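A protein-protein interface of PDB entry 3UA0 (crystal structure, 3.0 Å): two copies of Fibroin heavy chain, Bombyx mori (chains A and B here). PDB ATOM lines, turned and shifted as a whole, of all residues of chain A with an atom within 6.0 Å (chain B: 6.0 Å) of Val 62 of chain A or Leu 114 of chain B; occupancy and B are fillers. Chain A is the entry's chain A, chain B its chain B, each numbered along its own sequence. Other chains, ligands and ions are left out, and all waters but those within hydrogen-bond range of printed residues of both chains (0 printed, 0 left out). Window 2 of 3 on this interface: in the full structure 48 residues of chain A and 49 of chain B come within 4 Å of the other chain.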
ATOM      1  N   ILE A  54     -17.459   4.258  14.894  1.00  0.00           N
ATOM      2  CA  ILE A  54     -18.768   3.663  14.802  1.00  0.00           C
ATOM      3  C   ILE A  54     -18.940   2.653  15.927  1.00  0.00           C
ATOM      4  O   ILE A  54     -18.125   1.744  16.112  1.00  0.00           O
ATOM      5  CB  ILE A  54     -19.091   3.102  13.394  1.00  0.00           C
ATOM      6  CG1 ILE A  54     -19.058   4.232  12.359  1.00  0.00           C
ATOM      7  CG2 ILE A  54     -20.487   2.473  13.368  1.00  0.00           C
ATOM      8  CD1 ILE A  54     -20.262   5.153  12.420  1.00  0.00           C
ATOM      9  N   ILE A  55     -20.000   2.869  16.696  1.00  0.00           N
ATOM     10  CA  ILE A  55     -20.344   2.019  17.815  1.00  0.00           C
ATOM     11  C   ILE A  55     -21.626   1.253  17.496  1.00  0.00           C
ATOM     12  O   ILE A  55     -22.717   1.827  17.462  1.00  0.00           O
ATOM     13  CB  ILE A  55     -20.542   2.851  19.129  1.00  0.00           C
ATOM     14  CG1 ILE A  55     -19.208   3.381  19.662  1.00  0.00           C
ATOM     15  CG2 ILE A  55     -21.251   2.035  20.200  1.00  0.00           C
ATOM     16  CD1 ILE A  55     -18.902   4.800  19.238  1.00  0.00           C
ATOM     17  N   ARG A  56     -21.483  -0.040  17.221  1.00  0.00           N
ATOM     18  CA  ARG A  56     -22.616  -0.952  17.252  1.00  0.00           C
ATOM     19  C   ARG A  56     -22.639  -1.342  18.720  1.00  0.00           C
ATOM     20  O   ARG A  56     -21.584  -1.611  19.302  1.00  0.00           O
ATOM     21  CB  ARG A  56     -22.338  -2.175  16.368  1.00  0.00           C
ATOM     22  CG  ARG A  56     -23.549  -2.835  15.668  1.00  0.00           C
ATOM     23  CD  ARG A  56     -23.039  -3.706  14.492  1.00  0.00           C
ATOM     24  NE  ARG A  56     -23.975  -4.708  13.965  1.00  0.00           N
ATOM     25  CZ  ARG A  56     -23.612  -5.713  13.161  1.00  0.00           C
ATOM     26  NH1 ARG A  56     -22.336  -5.858  12.806  1.00  0.00           N
ATOM     27  NH2 ARG A  56     -24.515  -6.587  12.720  1.00  0.00           N
ATOM     28  N   ASP A  57     -23.809  -1.336  19.350  1.00  0.00           N
ATOM     29  CA  ASP A  57     -23.858  -1.698  20.765  1.00  0.00           C
ATOM     30  C   ASP A  57     -24.456  -3.082  21.002  1.00  0.00           C
ATOM     31  O   ASP A  57     -24.550  -3.903  20.083  1.00  0.00           O
ATOM     32  CB  ASP A  57     -24.558  -0.616  21.609  1.00  0.00           C
ATOM     33  CG  ASP A  57     -26.067  -0.563  21.391  1.00  0.00           C
ATOM     34  OD1 ASP A  57     -26.716  -1.620  21.334  1.00  0.00           O
ATOM     35  OD2 ASP A  57     -26.618   0.554  21.307  1.00  0.00           O
ATOM     36  N   GLY A  60     -27.093  -3.964  18.726  1.00  0.00           N
ATOM     37  CA  GLY A  60     -26.671  -3.763  17.354  1.00  0.00           C
ATOM     38  C   GLY A  60     -26.899  -2.331  16.916  1.00  0.00           C
ATOM     39  O   GLY A  60     -26.520  -1.950  15.805  1.00  0.00           O
ATOM     40  N   ALA A  61     -27.528  -1.545  17.789  1.00  0.00           N
ATOM     41  CA  ALA A  61     -27.786  -0.144  17.509  1.00  0.00           C
ATOM     42  C   ALA A  61     -26.467   0.536  17.179  1.00  0.00           C
ATOM     43  O   ALA A  61     -25.432   0.240  17.780  1.00  0.00           O
ATOM     44  CB  ALA A  61     -28.460   0.521  18.685  1.00  0.00           C
ATOM     45  N   VAL A  62     -26.508   1.434  16.204  1.00  0.00           N
ATOM     46  CA  VAL A  62     -25.282   1.976  15.644  1.00  0.00           C
ATOM     47  C   VAL A  62     -25.125   3.456  15.964  1.00  0.00           C
ATOM     48  O   VAL A  62     -26.056   4.239  15.796  1.00  0.00           O
ATOM     49  CB  VAL A  62     -25.220   1.727  14.122  1.00  0.00           C
ATOM     50  CG1 VAL A  62     -23.929   2.280  13.530  1.00  0.00           C
ATOM     51  CG2 VAL A  62     -25.350   0.243  13.845  1.00  0.00           C
ATOM     52  N   ILE A  63     -23.935   3.822  16.431  1.00  0.00           N
ATOM     53  CA  ILE A  63     -23.647   5.183  16.862  1.00  0.00           C
ATOM     54  C   ILE A  63     -22.429   5.707  16.136  1.00  0.00           C
ATOM     55  O   ILE A  63     -21.379   5.074  16.145  1.00  0.00           O
ATOM     56  CB  ILE A  63     -23.356   5.238  18.391  1.00  0.00           C
ATOM     57  CG1 ILE A  63     -24.629   4.971  19.192  1.00  0.00           C
ATOM     58  CG2 ILE A  63     -22.731   6.579  18.798  1.00  0.00           C
ATOM     59  CD1 ILE A  63     -24.376   4.222  20.466  1.00  0.00           C
ATOM     60  N   GLU A  64     -22.561   6.870  15.512  1.00  0.00           N
ATOM     61  CA  GLU A  64     -21.385   7.550  15.007  1.00  0.00           C
ATOM     62  C   GLU A  64     -20.871   8.543  16.047  1.00  0.00           C
ATOM     63  O   GLU A  64     -21.633   9.311  16.635  1.00  0.00           O
ATOM     64  CB  GLU A  64     -21.676   8.260  13.690  1.00  0.00           C
ATOM     65  CG  GLU A  64     -20.420   8.651  12.918  1.00  0.00           C
ATOM     66  CD  GLU A  64     -20.730   9.497  11.689  1.00  0.00           C
ATOM     67  OE1 GLU A  64     -21.711  10.270  11.740  1.00  0.00           O
ATOM     68  OE2 GLU A  64     -20.001   9.395  10.675  1.00  0.00           O
ATOM     69  N   LYS B 112     -24.214  10.963  17.310  1.00  0.00           N
ATOM     70  CA  LYS B 112     -25.524  10.674  16.760  1.00  0.00           C
ATOM     71  C   LYS B 112     -25.760   9.179  16.791  1.00  0.00           C
ATOM     72  O   LYS B 112     -24.823   8.389  16.868  1.00  0.00           O
ATOM     73  CB  LYS B 112     -25.687  11.231  15.335  1.00  0.00           C
ATOM     74  CG  LYS B 112     -24.388  11.442  14.556  1.00  0.00           C
ATOM     75  CD  LYS B 112     -24.630  12.303  13.308  1.00  0.00           C
ATOM     76  CE  LYS B 112     -23.327  12.776  12.646  1.00  0.00           C
ATOM     77  NZ  LYS B 112     -23.560  13.551  11.379  1.00  0.00           N
ATOM     78  N   THR B 113     -27.027   8.800  16.766  1.00  0.00           N
ATOM     79  CA  THR B 113     -27.393   7.409  16.591  1.00  0.00           C
ATOM     80  C   THR B 113     -27.885   7.175  15.161  1.00  0.00           C
ATOM     81  O   THR B 113     -28.856   7.794  14.711  1.00  0.00           O
ATOM     82  CB  THR B 113     -28.466   6.981  17.598  1.00  0.00           C
ATOM     83  OG1 THR B 113     -29.510   6.280  16.909  1.00  0.00           O
ATOM     84  CG2 THR B 113     -29.052   8.205  18.296  1.00  0.00           C
ATOM     85  N   LEU B 114     -27.185   6.297  14.445  1.00  0.00           N
ATOM     86  CA  LEU B 114     -27.571   5.884  13.102  1.00  0.00           C
ATOM     87  C   LEU B 114     -28.211   4.503  13.207  1.00  0.00           C
ATOM     88  O   LEU B 114     -27.729   3.649  13.956  1.00  0.00           O
ATOM     89  CB  LEU B 114     -26.334   5.790  12.218  1.00  0.00           C
ATOM     90  CG  LEU B 114     -25.128   6.645  12.606  1.00  0.00           C
ATOM     91  CD1 LEU B 114     -23.856   6.032  12.059  1.00  0.00           C
ATOM     92  CD2 LEU B 114     -25.293   8.064  12.119  1.00  0.00           C
ATOM     93  N   SER B 115     -29.306   4.290  12.485  1.00  0.00           N
ATOM     94  CA  SER B 115     -29.923   2.965  12.390  1.00  0.00           C
ATOM     95  C   SER B 115     -30.132   2.220  13.725  1.00  0.00           C
ATOM     96  O   SER B 115     -29.744   2.696  14.802  1.00  0.00           O
ATOM     97  CB  SER B 115     -29.111   2.088  11.428  1.00  0.00           C
ATOM     98  OG  SER B 115     -29.936   1.163  10.737  1.00  0.00           O
ATOM     99  N   ASP B 116     -30.744   1.039  13.619  1.00  0.00           N
ATOM    100  CA  ASP B 116     -31.088   0.172  14.760  1.00  0.00           C
ATOM    101  C   ASP B 116     -31.378   0.897  16.070  1.00  0.00           C
ATOM    102  O   ASP B 116     -32.378   0.609  16.723  1.00  0.00           O
ATOM    103  CB  ASP B 116     -30.035  -0.926  14.968  1.00  0.00           C
ATOM    104  CG  ASP B 116     -30.254  -2.123  14.050  1.00  0.00           C
ATOM    105  OD1 ASP B 116     -31.186  -2.075  13.213  1.00  0.00           O
ATOM    106  OD2 ASP B 116     -29.496  -3.113  14.168  1.00  0.00           O
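The backbone carbonyl oxygen (O) of Val 62 of chain A is in hydrogen-bond range of the backbone NH (N) of Leu 114 of chain B (2.7 Å). The side-chain amino group (NZ) of Lys 112 of chain B is in salt-bridge range of the side-chain carboxylate (OE1) of Glu 64 of chain A (3.8 Å).
The backbone carbonyl oxygen (O) of Ile 55 of chain A lies within hydrogen-bond range of the backbone NH (N) of Ile 63 of chain A (2.6 Å).
Ile 54 of chain A touches Leu 114 of chain B (CD1 to CD1, 3.7 Å). Gly 60 of chain A touches Asp 116 of chain B. CA of Ala 61 of chain A touches CB of Asp 116 of chain B, 3.5 Å away. Val 62 of chain A touches Thr 113 of chain B (O to C, 3.5 Å). Val 62 of chain A touches Ser 115 of chain B (N to O, 3.7 Å). CG2 of Ile 63 of chain A touches O of Lys 112 of chain B (3.4 Å). CB of Glu 64 of chain A touches CD1 of Leu 114 of chain B, 3.5 Å away.
Of the printed residues of chain B, Val 62 of chain A touches Thr 113, Leu 114 and Ser 115. Of the printed residues of chain B, Ile 63 of chain A touches Lys 112. Printed residues of chain A within 4 Å of Thr 113 of chain B: Val 62. Printed residues of chain A within 4 Å of Leu 114 of chain B: Ile 54 (3.7 Å), Val 62 (2.6 Å) and Glu 64 (3.5 Å). Of the printed residues of chain A, Asp 116 of chain B touches Gly 60 (3.6 Å) and Ala 61 (3.5 Å). The nearest residue of chain B that does not touch Val 62 of chain A is Asp 116 of chain B (4.4 Å).
Hydrophobic or aromatic side chains of chain B within 4 Å of the printed part of chain A: Leu 114. Hydrophobic or aromatic side chains of chain A that line the printed part of chain B: Ile 54, Ala 61, Val 62 and Ile 63. Among the printed residues, 9 pairs touch across the chains. Among the printed residues, Asp or Glu carboxylates within 4 Å of a Lys or Arg side-chain nitrogen of the other chain: Glu 64 of chain A with Lys 112 of chain B (3.8 Å).
No position is printed for both chains. Of the 9 pairs that touch across the chains among the printed residues, none has its exchanged pair printed and touching as well.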
